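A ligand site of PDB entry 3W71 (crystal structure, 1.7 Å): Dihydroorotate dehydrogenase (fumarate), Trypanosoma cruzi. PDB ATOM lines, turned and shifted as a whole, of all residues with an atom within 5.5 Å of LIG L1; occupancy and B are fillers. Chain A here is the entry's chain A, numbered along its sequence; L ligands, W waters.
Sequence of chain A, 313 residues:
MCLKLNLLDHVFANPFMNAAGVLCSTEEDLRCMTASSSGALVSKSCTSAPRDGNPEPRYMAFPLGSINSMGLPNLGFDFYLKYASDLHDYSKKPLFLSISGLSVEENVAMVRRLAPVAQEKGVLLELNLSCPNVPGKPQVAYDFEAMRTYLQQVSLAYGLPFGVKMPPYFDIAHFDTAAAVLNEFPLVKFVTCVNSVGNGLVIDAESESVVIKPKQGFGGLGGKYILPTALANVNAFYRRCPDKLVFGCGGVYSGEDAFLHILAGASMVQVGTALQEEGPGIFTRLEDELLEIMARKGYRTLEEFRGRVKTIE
The side-chain hydroxyl of Thr 273 lies within hydrogen-bond range of the side-chain hydroxyl of Ser 66 (2.8 Å). The backbone NH of Val 194 lies within hydrogen-bond range of the backbone carbonyl oxygen of Cys 249 (2.9 Å). The side-chain amide oxygen (OE1) of Gln 270 is in hydrogen-bond range of the side-chain sulfur (SG) of Cys 249 (3.7 Å). The backbone carbonyl oxygen (O) of Gly 222 is in hydrogen-bond range of the backbone NH (N) of Ser 66, 3.0 Å away. The backbone NH (N) of Met 70 lies within hydrogen-bond range of the side-chain amide oxygen (OD1) of Asn 68 (3.3 Å). OD1 of Asn 128 lies within hydrogen-bond range of ND2 of Asn 195 (3.4 Å). OD1 of Asn 195 lies within hydrogen-bond range of OG of Ser 196, 3.3 Å away. The backbone carbonyl oxygen (O) of Val 271 lies within hydrogen-bond range of the backbone NH (N) of Ala 19, 2.9 Å away.
N2 of LG2 L2 sits close to N1 of LIG L1 (3.4 Å).
The side-chain amino group (NZ) of Lys 44 lies within hydrogen-bond range of an oxygen (O2) of LIG L1 (2.8 Å). OG of Ser 196 is in hydrogen-bond range of O3 of LG2 L2 (2.8 Å). A nitrogen (N2) of LIG L1 sits at hydrogen-bond distance from the side-chain hydroxyl of Ser 45 (2.7 Å). An oxygen (O3) of LIG L1 lies within hydrogen-bond range of the backbone carbonyl oxygen of Ala 20 (2.8 Å). The backbone carbonyl oxygen (O) of Val 194 lies within hydrogen-bond range of an oxygen (O4) of LIG L1 (2.9 Å). SG of Cys 249 lies within hydrogen-bond range of O4 of LIG L1 (3.5 Å). An oxygen (O4) of LG2 L2 sits at hydrogen-bond distance from the side-chain amide nitrogen (ND2) of Asn 128 (2.9 Å). N of Gly 223 sits at hydrogen-bond distance from O8 of LIG L1 (2.7 Å). An oxygen (O2) of LG2 L2 is in hydrogen-bond range of the backbone NH (N) of Leu 72 (2.9 Å). O1 of LIG L1 is in hydrogen-bond range of ND2 of Asn 128 (3.3 Å). The backbone NH (N) of Gly 272 sits at hydrogen-bond distance from an oxygen (O7) of LIG L1, 2.9 Å away. N2 of LG2 L2 is in hydrogen-bond range of OD1 of Asn 195 (2.8 Å). The side-chain amino group (NZ) of Lys 165 is in hydrogen-bond range of an oxygen (O3) of LIG L1 (2.9 Å). The side-chain hydroxyl of Thr 273 is in hydrogen-bond range of an oxygen (O9) of LIG L1 (2.7 Å). N of Thr 273 lies within hydrogen-bond range of O9 of LIG L1 (2.8 Å). O2 of LG2 L2 lies within salt-bridge range of NZ of Lys 44 (3.1 Å). The backbone NH (N) of Met 70 lies within hydrogen-bond range of an oxygen (O1) of LG2 L2 (3.1 Å). ND2 of Asn 68 is in hydrogen-bond range of O3 of LG2 L2, at 2.9 Å. The side-chain amide nitrogen (ND2) of Asn 195 lies within hydrogen-bond range of an oxygen (O1) of LIG L1 (3.4 Å). An oxygen (O8) of LIG L1 sits at hydrogen-bond distance from the backbone NH of Gly 251, at 2.8 Å. An oxygen (O3) of LIG L1 sits at hydrogen-bond distance from the backbone NH of Ala 20 (3.5 Å).
Water W2 lies within hydrogen-bond range of an oxygen (O7) of LIG L1, the backbone NH of Ala 274, the backbone carbonyl oxygen of Val 252 and the backbone NH of Thr 273. Water W5 lies within hydrogen-bond range of OG of Ser 98 (2.6 Å), OE1 of Glu 126 (2.7 Å) and O1 of LIG L1 (2.8 Å). Water W1 lies within hydrogen-bond range of NZ of Lys 44 (3.0 Å) and O of Gly 21 (3.1 Å).
Ala 19 touches LIG L1. Gly 21 touches LIG L1. Tyr 59 touches LIG L1. Asn 68 touches LIG L1 (ND2 to C8, 3.5 Å). CG of Met 70 touches C7 of LIG L1, at 3.8 Å. Ser 196 touches LIG L1. Gly 222 touches LIG L1 (C to O8, 3.7 Å). CD1 of Ile 226 touches O8 of LIG L1, 3.7 Å away. CA of Gly 250 touches O8 of LIG L1, at 3.4 Å. 21 residues have an atom within 4 Å of LIG L1: Ala 19, Ala 20, Gly 21, Lys 44, Ser 45, Tyr 59, Asn 68, Met 70, Asn 128, Lys 165, Val 194, Asn 195, Ser 196, Gly 222, Gly 223, Ile 226, Cys 249, Gly 250, Gly 251, Gly 272 and Thr 273. The nearest printed residue that does not touch LIG L1 is Val 271 (4.04 Å).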
ATOM      1  N   ALA A  19      25.134 -22.740 -31.236  1.00  0.00           N
ATOM      2  CA  ALA A  19      24.542 -21.898 -30.238  1.00  0.00           C
ATOM      3  C   ALA A  19      25.311 -21.930 -28.902  1.00  0.00           C
ATOM      4  O   ALA A  19      25.822 -22.940 -28.512  1.00  0.00           O
ATOM      5  CB  ALA A  19      23.131 -22.328 -30.025  1.00  0.00           C
ATOM      6  N   ALA A  20      25.351 -20.844 -28.167  1.00  0.00           N
ATOM      7  CA  ALA A  20      26.087 -20.837 -26.962  1.00  0.00           C
ATOM      8  C   ALA A  20      25.516 -21.926 -26.039  1.00  0.00           C
ATOM      9  O   ALA A  20      24.276 -22.125 -25.983  1.00  0.00           O
ATOM     10  CB  ALA A  20      25.991 -19.472 -26.256  1.00  0.00           C
ATOM     11  N   GLY A  21      26.414 -22.619 -25.346  1.00  0.00           N
ATOM     12  CA  GLY A  21      26.045 -23.637 -24.445  1.00  0.00           C
ATOM     13  C   GLY A  21      26.226 -25.013 -25.058  1.00  0.00           C
ATOM     14  O   GLY A  21      26.335 -26.027 -24.302  1.00  0.00           O
ATOM     15  N   VAL A  22      26.106 -25.122 -26.366  1.00  0.00           N
ATOM     16  CA  VAL A  22      26.206 -26.457 -27.026  1.00  0.00           C
ATOM     17  C   VAL A  22      27.595 -26.620 -27.542  1.00  0.00           C
ATOM     18  O   VAL A  22      28.082 -25.821 -28.341  1.00  0.00           O
ATOM     19  CB  VAL A  22      25.125 -26.564 -28.079  1.00  0.00           C
ATOM     20  CG1 VAL A  22      25.269 -27.867 -28.859  1.00  0.00           C
ATOM     21  CG2 VAL A  22      23.780 -26.397 -27.387  1.00  0.00           C
ATOM     22  N   LYS A  44      30.768 -21.295 -24.223  1.00  0.00           N
ATOM     23  CA  LYS A  44      29.757 -21.356 -23.187  1.00  0.00           C
ATOM     24  C   LYS A  44      29.720 -20.043 -22.418  1.00  0.00           C
ATOM     25  O   LYS A  44      30.763 -19.526 -22.040  1.00  0.00           O
ATOM     26  CB  LYS A  44      30.171 -22.439 -22.240  1.00  0.00           C
ATOM     27  CG  LYS A  44      29.268 -22.616 -21.060  1.00  0.00           C
ATOM     28  CD  LYS A  44      27.804 -22.934 -21.271  1.00  0.00           C
ATOM     29  CE  LYS A  44      26.932 -22.710 -20.043  1.00  0.00           C
ATOM     30  NZ  LYS A  44      25.464 -23.082 -20.299  1.00  0.00           N
ATOM     31  N   SER A  45      28.513 -19.540 -22.206  1.00  0.00           N
ATOM     32  CA  SER A  45      28.286 -18.329 -21.383  1.00  0.00           C
ATOM     33  C   SER A  45      29.019 -18.586 -20.090  1.00  0.00           C
ATOM     34  O   SER A  45      28.838 -19.606 -19.430  1.00  0.00           O
ATOM     35  CB  SER A  45      26.847 -18.050 -21.135  1.00  0.00           C
ATOM     36  OG  SER A  45      26.207 -17.686 -22.315  1.00  0.00           O
ATOM     37  N   TYR A  59      19.256 -31.791 -18.837  1.00  0.00           N
ATOM     38  CA  TYR A  59      18.991 -31.672 -20.260  1.00  0.00           C
ATOM     39  C   TYR A  59      18.357 -32.934 -20.744  1.00  0.00           C
ATOM     40  O   TYR A  59      18.886 -34.036 -20.430  1.00  0.00           O
ATOM     41  CB  TYR A  59      20.267 -31.425 -21.092  1.00  0.00           C
ATOM     42  CG  TYR A  59      20.134 -31.524 -22.615  1.00  0.00           C
ATOM     43  CD1 TYR A  59      20.300 -32.701 -23.275  1.00  0.00           C
ATOM     44  CD2 TYR A  59      19.751 -30.420 -23.393  1.00  0.00           C
ATOM     45  CE1 TYR A  59      20.071 -32.785 -24.644  1.00  0.00           C
ATOM     46  CE2 TYR A  59      19.542 -30.484 -24.738  1.00  0.00           C
ATOM     47  CZ  TYR A  59      19.749 -31.702 -25.388  1.00  0.00           C
ATOM     48  OH  TYR A  59      19.541 -31.774 -26.739  1.00  0.00           O
ATOM     49  N   SER A  66      14.181 -29.913 -27.176  1.00  0.00           N
ATOM     50  CA  SER A  66      14.869 -30.192 -25.961  1.00  0.00           C
ATOM     51  C   SER A  66      14.327 -29.249 -24.840  1.00  0.00           C
ATOM     52  O   SER A  66      13.692 -28.233 -25.083  1.00  0.00           O
ATOM     53  CB  SER A  66      16.380 -29.954 -26.114  1.00  0.00           C
ATOM     54  OG  SER A  66      16.605 -28.530 -26.314  1.00  0.00           O
ATOM     55  N   ASN A  68      16.014 -27.754 -20.999  1.00  0.00           N
ATOM     56  CA  ASN A  68      17.198 -27.680 -20.199  1.00  0.00           C
ATOM     57  C   ASN A  68      17.056 -26.722 -19.027  1.00  0.00           C
ATOM     58  O   ASN A  68      16.491 -25.618 -19.146  1.00  0.00           O
ATOM     59  CB  ASN A  68      18.488 -27.352 -21.025  1.00  0.00           C
ATOM     60  CG  ASN A  68      18.743 -25.889 -21.137  1.00  0.00           C
ATOM     61  OD1 ASN A  68      19.354 -25.260 -20.243  1.00  0.00           O
ATOM     62  ND2 ASN A  68      18.397 -25.338 -22.238  1.00  0.00           N
ATOM     63  N   MET A  70      20.390 -26.082 -17.250  1.00  0.00           N
ATOM     64  CA  MET A  70      21.782 -26.439 -16.966  1.00  0.00           C
ATOM     65  C   MET A  70      22.300 -25.653 -15.736  1.00  0.00           C
ATOM     66  O   MET A  70      23.115 -26.166 -14.939  1.00  0.00           O
ATOM     67  CB  MET A  70      22.609 -26.085 -18.145  1.00  0.00           C
ATOM     68  CG  MET A  70      22.326 -26.714 -19.455  1.00  0.00           C
ATOM     69  SD  MET A  70      22.253 -28.490 -19.461  1.00  0.00           S
ATOM     70  CE  MET A  70      23.914 -28.923 -19.283  1.00  0.00           C
ATOM     71  N   LEU A  72      24.131 -22.716 -15.888  1.00  0.00           N
ATOM     72  CA  LEU A  72      25.391 -22.113 -16.244  1.00  0.00           C
ATOM     73  C   LEU A  72      26.610 -22.839 -15.684  1.00  0.00           C
ATOM     74  O   LEU A  72      27.619 -22.237 -15.201  1.00  0.00           O
ATOM     75  CB  LEU A  72      25.375 -20.636 -15.739  1.00  0.00           C
ATOM     76  CG  LEU A  72      25.842 -19.415 -16.488  1.00  0.00           C
ATOM     77  CD1 LEU A  72      25.646 -19.360 -17.992  1.00  0.00           C
ATOM     78  CD2 LEU A  72      25.223 -18.175 -15.729  1.00  0.00           C
ATOM     79  N   SER A  98      30.949 -15.743 -25.091  1.00  0.00           N
ATOM     80  CA  SER A  98      29.683 -15.366 -24.474  1.00  0.00           C
ATOM     81  C   SER A  98      29.869 -15.209 -22.983  1.00  0.00           C
ATOM     82  O   SER A  98      30.514 -16.030 -22.345  1.00  0.00           O
ATOM     83  CB  SER A  98      28.604 -16.432 -24.752  1.00  0.00           C
ATOM     84  OG  SER A  98      27.408 -16.074 -24.031  1.00  0.00           O
ATOM     85  N   GLU A 126      29.659 -11.727 -27.101  1.00  0.00           N
ATOM     86  CA  GLU A 126      28.175 -11.945 -27.103  1.00  0.00           C
ATOM     87  C   GLU A 126      27.749 -11.851 -25.601  1.00  0.00           C
ATOM     88  O   GLU A 126      28.090 -12.675 -24.777  1.00  0.00           O
ATOM     89  CB  GLU A 126      27.712 -13.283 -27.733  1.00  0.00           C
ATOM     90  CG  GLU A 126      26.169 -13.416 -27.794  1.00  0.00           C
ATOM     91  CD  GLU A 126      25.687 -14.682 -28.625  1.00  0.00           C
ATOM     92  OE1 GLU A 126      25.621 -15.762 -28.013  1.00  0.00           O
ATOM     93  OE2 GLU A 126      25.438 -14.739 -29.909  1.00  0.00           O
ATOM     94  N   ASN A 128      25.030 -12.275 -22.876  1.00  0.00           N
ATOM     95  CA  ASN A 128      23.796 -12.965 -22.695  1.00  0.00           C
ATOM     96  C   ASN A 128      22.878 -12.201 -21.724  1.00  0.00           C
ATOM     97  O   ASN A 128      23.152 -12.166 -20.495  1.00  0.00           O
ATOM     98  CB  ASN A 128      24.102 -14.342 -22.089  1.00  0.00           C
ATOM     99  CG  ASN A 128      22.885 -15.215 -21.994  1.00  0.00           C
ATOM    100  OD1 ASN A 128      21.803 -14.838 -22.256  1.00  0.00           O
ATOM    101  ND2 ASN A 128      23.139 -16.459 -21.516  1.00  0.00           N
ATOM    102  N   LYS A 165      22.684 -11.524 -26.789  1.00  0.00           N
ATOM    103  CA  LYS A 165      21.788 -12.716 -26.975  1.00  0.00           C
ATOM    104  C   LYS A 165      20.489 -12.396 -26.203  1.00  0.00           C
ATOM    105  O   LYS A 165      20.473 -12.081 -25.032  1.00  0.00           O
ATOM    106  CB  LYS A 165      22.452 -13.918 -26.377  1.00  0.00           C
ATOM    107  CG  LYS A 165      21.632 -15.241 -26.362  1.00  0.00           C
ATOM    108  CD  LYS A 165      21.596 -15.819 -27.755  1.00  0.00           C
ATOM    109  CE  LYS A 165      21.061 -17.221 -27.676  1.00  0.00           C
ATOM    110  NZ  LYS A 165      22.014 -18.216 -27.214  1.00  0.00           N
ATOM    111  N   VAL A 194      17.006 -16.388 -31.077  1.00  0.00           N
ATOM    112  CA  VAL A 194      16.612 -16.229 -29.708  1.00  0.00           C
ATOM    113  C   VAL A 194      17.294 -17.256 -28.831  1.00  0.00           C
ATOM    114  O   VAL A 194      17.754 -18.333 -29.229  1.00  0.00           O
ATOM    115  CB  VAL A 194      15.061 -16.402 -29.473  1.00  0.00           C
ATOM    116  CG1 VAL A 194      14.343 -15.338 -30.227  1.00  0.00           C
ATOM    117  CG2 VAL A 194      14.620 -17.779 -30.008  1.00  0.00           C
ATOM    118  N   ASN A 195      17.383 -16.915 -27.549  1.00  0.00           N
ATOM    119  CA  ASN A 195      17.596 -17.929 -26.461  1.00  0.00           C
ATOM    120  C   ASN A 195      16.396 -18.903 -26.322  1.00  0.00           C
ATOM    121  O   ASN A 195      15.363 -18.780 -27.013  1.00  0.00           O
ATOM    122  CB  ASN A 195      17.924 -17.179 -25.151  1.00  0.00           C
ATOM    123  CG  ASN A 195      18.885 -17.928 -24.261  1.00  0.00           C
ATOM    124  OD1 ASN A 195      18.776 -19.118 -24.066  1.00  0.00           O
ATOM    125  ND2 ASN A 195      19.939 -17.221 -23.807  1.00  0.00           N
ATOM    126  N   SER A 196      16.502 -19.868 -25.406  1.00  0.00           N
ATOM    127  CA  SER A 196      15.402 -20.820 -25.184  1.00  0.00           C
ATOM    128  C   SER A 196      14.103 -20.157 -24.839  1.00  0.00           C
ATOM    129  O   SER A 196      14.087 -19.061 -24.212  1.00  0.00           O
ATOM    130  CB  SER A 196      15.919 -21.883 -24.189  1.00  0.00           C
ATOM    131  OG  SER A 196      16.380 -21.234 -23.081  1.00  0.00           O
ATOM    132  N   LEU A 221      13.100 -24.319 -23.503  1.00  0.00           N
ATOM    133  CA  LEU A 221      12.815 -25.180 -24.645  1.00  0.00           C
ATOM    134  C   LEU A 221      13.618 -24.679 -25.847  1.00  0.00           C
ATOM    135  O   LEU A 221      13.726 -23.496 -26.140  1.00  0.00           O
ATOM    136  CB  LEU A 221      11.333 -25.040 -25.004  1.00  0.00           C
ATOM    137  CG  LEU A 221      10.302 -25.386 -23.938  1.00  0.00           C
ATOM    138  CD1 LEU A 221       8.876 -25.007 -24.456  1.00  0.00           C
ATOM    139  CD2 LEU A 221      10.402 -26.811 -23.432  1.00  0.00           C
ATOM    140  N   GLY A 222      14.078 -25.635 -26.608  1.00  0.00           N
ATOM    141  CA  GLY A 222      14.696 -25.452 -27.884  1.00  0.00           C
ATOM    142  C   GLY A 222      14.197 -26.474 -28.920  1.00  0.00           C
ATOM    143  O   GLY A 222      13.473 -27.413 -28.591  1.00  0.00           O
ATOM    144  N   GLY A 223      14.621 -26.283 -30.147  1.00  0.00           N
ATOM    145  CA  GLY A 223      14.386 -27.232 -31.207  1.00  0.00           C
ATOM    146  C   GLY A 223      13.130 -26.908 -32.013  1.00  0.00           C
ATOM    147  O   GLY A 223      12.731 -25.763 -32.167  1.00  0.00           O
ATOM    148  N   ILE A 226      10.311 -24.315 -31.271  1.00  0.00           N
ATOM    149  CA  ILE A 226      10.498 -22.920 -31.229  1.00  0.00           C
ATOM    150  C   ILE A 226      10.787 -22.177 -32.550  1.00  0.00           C
ATOM    151  O   ILE A 226      11.009 -20.968 -32.553  1.00  0.00           O
ATOM    152  CB  ILE A 226      11.559 -22.546 -30.145  1.00  0.00           C
ATOM    153  CG1 ILE A 226      12.995 -22.664 -30.618  1.00  0.00           C
ATOM    154  CG2 ILE A 226      11.298 -23.306 -28.833  1.00  0.00           C
ATOM    155  CD1 ILE A 226      14.000 -21.924 -29.763  1.00  0.00           C
ATOM    156  N   CYS A 249      18.825 -17.860 -34.176  1.00  0.00           N
ATOM    157  CA  CYS A 249      19.036 -19.124 -33.400  1.00  0.00           C
ATOM    158  C   CYS A 249      17.662 -19.635 -33.025  1.00  0.00           C
ATOM    159  O   CYS A 249      16.830 -18.841 -32.546  1.00  0.00           O
ATOM    160  CB  CYS A 249      19.858 -18.783 -32.152  1.00  0.00           C
ATOM    161  SG  CYS A 249      20.307 -20.241 -31.180  1.00  0.00           S
ATOM    162  N   GLY A 250      17.379 -20.904 -33.280  1.00  0.00           N
ATOM    163  CA  GLY A 250      16.165 -21.619 -32.790  1.00  0.00           C
ATOM    164  C   GLY A 250      15.570 -22.469 -33.856  1.00  0.00           C
ATOM    165  O   GLY A 250      15.208 -21.967 -34.939  1.00  0.00           O
ATOM    166  N   GLY A 251      15.502 -23.741 -33.534  1.00  0.00           N
ATOM    167  CA  GLY A 251      14.825 -24.651 -34.459  1.00  0.00           C
ATOM    168  C   GLY A 251      15.519 -25.007 -35.696  1.00  0.00           C
ATOM    169  O   GLY A 251      14.823 -25.511 -36.565  1.00  0.00           O
ATOM    170  N   VAL A 252      16.817 -24.734 -35.843  1.00  0.00           N
ATOM    171  CA  VAL A 252      17.462 -25.110 -37.106  1.00  0.00           C
ATOM    172  C   VAL A 252      17.884 -26.606 -37.038  1.00  0.00           C
ATOM    173  O   VAL A 252      18.804 -26.959 -36.296  1.00  0.00           O
ATOM    174  CB  VAL A 252      18.689 -24.207 -37.427  1.00  0.00           C
ATOM    175  CG1 VAL A 252      19.464 -24.686 -38.638  1.00  0.00           C
ATOM    176  CG2 VAL A 252      18.200 -22.753 -37.545  1.00  0.00           C
ATOM    177  N   GLN A 270      22.747 -19.929 -35.867  1.00  0.00           N
ATOM    178  CA  GLN A 270      23.326 -20.709 -34.790  1.00  0.00           C
ATOM    179  C   GLN A 270      22.442 -21.995 -34.670  1.00  0.00           C
ATOM    180  O   GLN A 270      21.212 -21.991 -34.920  1.00  0.00           O
ATOM    181  CB  GLN A 270      23.289 -19.964 -33.453  1.00  0.00           C
ATOM    182  CG  GLN A 270      23.858 -18.596 -33.603  1.00  0.00           C
ATOM    183  CD  GLN A 270      24.112 -17.942 -32.278  1.00  0.00           C
ATOM    184  OE1 GLN A 270      23.407 -18.267 -31.317  1.00  0.00           O
ATOM    185  NE2 GLN A 270      25.028 -16.975 -32.224  1.00  0.00           N
ATOM    186  N   VAL A 271      23.062 -23.103 -34.234  1.00  0.00           N
ATOM    187  CA  VAL A 271      22.466 -24.397 -34.088  1.00  0.00           C
ATOM    188  C   VAL A 271      22.756 -24.958 -32.702  1.00  0.00           C
ATOM    189  O   VAL A 271      23.918 -25.121 -32.325  1.00  0.00           O
ATOM    190  CB  VAL A 271      23.075 -25.355 -35.146  1.00  0.00           C
ATOM    191  CG1 VAL A 271      22.315 -26.639 -35.169  1.00  0.00           C
ATOM    192  CG2 VAL A 271      23.121 -24.689 -36.546  1.00  0.00           C
ATOM    193  N   GLY A 272      21.707 -25.158 -31.949  1.00  0.00           N
ATOM    194  CA  GLY A 272      21.762 -25.646 -30.541  1.00  0.00           C
ATOM    195  C   GLY A 272      21.368 -27.100 -30.468  1.00  0.00           C
ATOM    196  O   GLY A 272      22.182 -27.986 -30.610  1.00  0.00           O
ATOM    197  N   THR A 273      20.071 -27.325 -30.213  1.00  0.00           N
ATOM    198  CA  THR A 273      19.512 -28.667 -29.993  1.00  0.00           C
ATOM    199  C   THR A 273      19.952 -29.648 -31.080  1.00  0.00           C
ATOM    200  O   THR A 273      20.377 -30.687 -30.776  1.00  0.00           O
ATOM    201  CB  THR A 273      17.975 -28.640 -29.913  1.00  0.00           C
ATOM    202  OG1 THR A 273      17.552 -27.794 -28.804  1.00  0.00           O
ATOM    203  CG2 THR A 273      17.387 -29.972 -29.673  1.00  0.00           C
ATOM    204  N   ALA A 274      19.821 -29.256 -32.328  1.00  0.00           N
ATOM    205  CA  ALA A 274      20.131 -30.251 -33.383  1.00  0.00           C
ATOM    206  C   ALA A 274      21.586 -30.624 -33.378  1.00  0.00           C
ATOM    207  O   ALA A 274      21.933 -31.732 -33.773  1.00  0.00           O
ATOM    208  CB  ALA A 274      19.734 -29.633 -34.750  1.00  0.00           C
ATOM    209  N   GLN A 276      23.533 -30.563 -30.565  1.00  0.00           N
ATOM    210  CA  GLN A 276      23.592 -31.413 -29.372  1.00  0.00           C
ATOM    211  C   GLN A 276      23.159 -32.838 -29.744  1.00  0.00           C
ATOM    212  O   GLN A 276      23.812 -33.784 -29.333  1.00  0.00           O
ATOM    213  CB  GLN A 276      22.776 -30.875 -28.271  1.00  0.00           C
ATOM    214  CG  GLN A 276      22.832 -31.699 -27.044  1.00  0.00           C
ATOM    215  CD  GLN A 276      24.215 -31.872 -26.494  1.00  0.00           C
ATOM    216  OE1 GLN A 276      24.532 -32.967 -25.878  1.00  0.00           O
ATOM    217  NE2 GLN A 276      24.919 -30.811 -26.411  1.00  0.00           N
HETATM  218  N1  LIG L   1      22.251 -19.793 -24.499  1.00  0.00           N
HETATM  219  C1  LIG L   1      23.198 -18.914 -24.092  1.00  0.00           C
HETATM  220  O1  LIG L   1      23.176 -17.758 -24.550  1.00  0.00           O
HETATM  221  N2  LIG L   1      24.157 -19.242 -23.186  1.00  0.00           N
HETATM  222  C2  LIG L   1      24.304 -20.531 -22.721  1.00  0.00           C
HETATM  223  O2  LIG L   1      25.256 -20.870 -21.925  1.00  0.00           O
HETATM  224  C3  LIG L   1      23.355 -21.548 -23.118  1.00  0.00           C
HETATM  225  N3  LIG L   1      23.382 -22.822 -22.662  1.00  0.00           N
HETATM  226  C4  LIG L   1      22.626 -23.804 -23.266  1.00  0.00           C
HETATM  227  C5  LIG L   1      22.848 -25.151 -22.962  1.00  0.00           C
HETATM  228  C6  LIG L   1      21.987 -26.088 -23.494  1.00  0.00           C
HETATM  229  C7  LIG L   1      22.203 -27.539 -23.123  1.00  0.00           C
HETATM  230  C8  LIG L   1      21.027 -25.683 -24.460  1.00  0.00           C
HETATM  231  C9  LIG L   1      20.143 -26.680 -25.085  1.00  0.00           C
HETATM  232  C10 LIG L   1      20.820 -24.361 -24.780  1.00  0.00           C
HETATM  233  C11 LIG L   1      21.592 -23.389 -24.197  1.00  0.00           C
HETATM  234  N4  LIG L   1      21.430 -22.012 -24.545  1.00  0.00           N
HETATM  235  C12 LIG L   1      22.311 -21.094 -24.092  1.00  0.00           C
HETATM  236  C13 LIG L   1      20.442 -21.624 -25.524  1.00  0.00           C
HETATM  237  C14 LIG L   1      20.924 -21.867 -26.942  1.00  0.00           C
HETATM  238  O3  LIG L   1      22.039 -21.096 -27.215  1.00  0.00           O
HETATM  239  C15 LIG L   1      19.829 -21.547 -27.933  1.00  0.00           C
HETATM  240  O4  LIG L   1      19.513 -20.142 -27.806  1.00  0.00           O
HETATM  241  C16 LIG L   1      18.525 -22.361 -27.695  1.00  0.00           C
HETATM  242  O5  LIG L   1      18.834 -23.743 -27.424  1.00  0.00           O
HETATM  243  C17 LIG L   1      17.675 -22.381 -28.995  1.00  0.00           C
HETATM  244  O6  LIG L   1      18.284 -22.885 -30.158  1.00  0.00           O
HETATM  245  P1  LIG L   1      17.912 -24.368 -30.691  1.00  0.00           P
HETATM  246  O7  LIG L   1      18.816 -24.604 -31.865  1.00  0.00           O
HETATM  247  O8  LIG L   1      16.455 -24.418 -30.945  1.00  0.00           O
HETATM  248  O9  LIG L   1      18.233 -25.292 -29.518  1.00  0.00           O
HETATM  249  O1  LG2 L   2      20.909 -23.194 -18.102  1.00  0.00           O
HETATM  250  C1  LG2 L   2      21.765 -22.568 -18.748  1.00  0.00           C
HETATM  251  O2  LG2 L   2      23.025 -22.565 -18.525  1.00  0.00           O
HETATM  252  C2  LG2 L   2      21.225 -21.729 -19.860  1.00  0.00           C
HETATM  253  N1  LG2 L   2      20.296 -22.457 -20.692  1.00  0.00           N
HETATM  254  C3  LG2 L   2      19.665 -21.836 -21.752  1.00  0.00           C
HETATM  255  O3  LG2 L   2      18.812 -22.454 -22.437  1.00  0.00           O
HETATM  256  N2  LG2 L   2      20.077 -20.555 -22.015  1.00  0.00           N
HETATM  257  C4  LG2 L   2      20.916 -19.773 -21.213  1.00  0.00           C
HETATM  258  O4  LG2 L   2      21.169 -18.586 -21.543  1.00  0.00           O
HETATM  259  C5  LG2 L   2      21.552 -20.439 -20.123  1.00  0.00           C
HETATM  260  C6  LG2 L   2      22.411 -19.637 -19.298  1.00  0.00           C
HETATM  261  C7  LG2 L   2      21.617 -18.581 -18.505  1.00  0.00           C
HETATM  262  C8  LG2 L   2      21.069 -19.176 -17.311  1.00  0.00           C
HETATM  263  C9  LG2 L   2      21.620 -19.010 -16.066  1.00  0.00           C
HETATM  264  C10 LG2 L   2      21.088 -19.671 -14.898  1.00  0.00           C
HETATM  265  C11 LG2 L   2      19.916 -20.019 -17.311  1.00  0.00           C
HETATM  266  C12 LG2 L   2      19.387 -20.690 -16.182  1.00  0.00           C
HETATM  267  C13 LG2 L   2      19.963 -20.524 -14.901  1.00  0.00           C
HETATM  268  C14 LG2 L   2      19.410 -21.181 -13.740  1.00  0.00           C
HETATM  269  C15 LG2 L   2      20.123 -21.211 -12.518  1.00  0.00           C
HETATM  270  C16 LG2 L   2      19.573 -21.853 -11.398  1.00  0.00           C
HETATM  271  C17 LG2 L   2      18.338 -22.498 -11.502  1.00  0.00           C
HETATM  272  C18 LG2 L   2      17.649 -22.566 -12.684  1.00  0.00           C
HETATM  273  C19 LG2 L   2      18.171 -21.890 -13.802  1.00  0.00           C
HETATM  274  O   HOH W   1      25.774 -25.923 -21.213  1.00  0.00           O
HETATM  275  O   HOH W   2      18.598 -26.818 -33.298  1.00  0.00           O
HETATM  276  O   HOH W   3      17.264 -24.272 -25.604  1.00  0.00           O
HETATM  277  O   HOH W   4      18.828 -23.222 -34.146  1.00  0.00           O
HETATM  278  O   HOH W   5      25.178 -15.904 -25.325  1.00  0.00           O
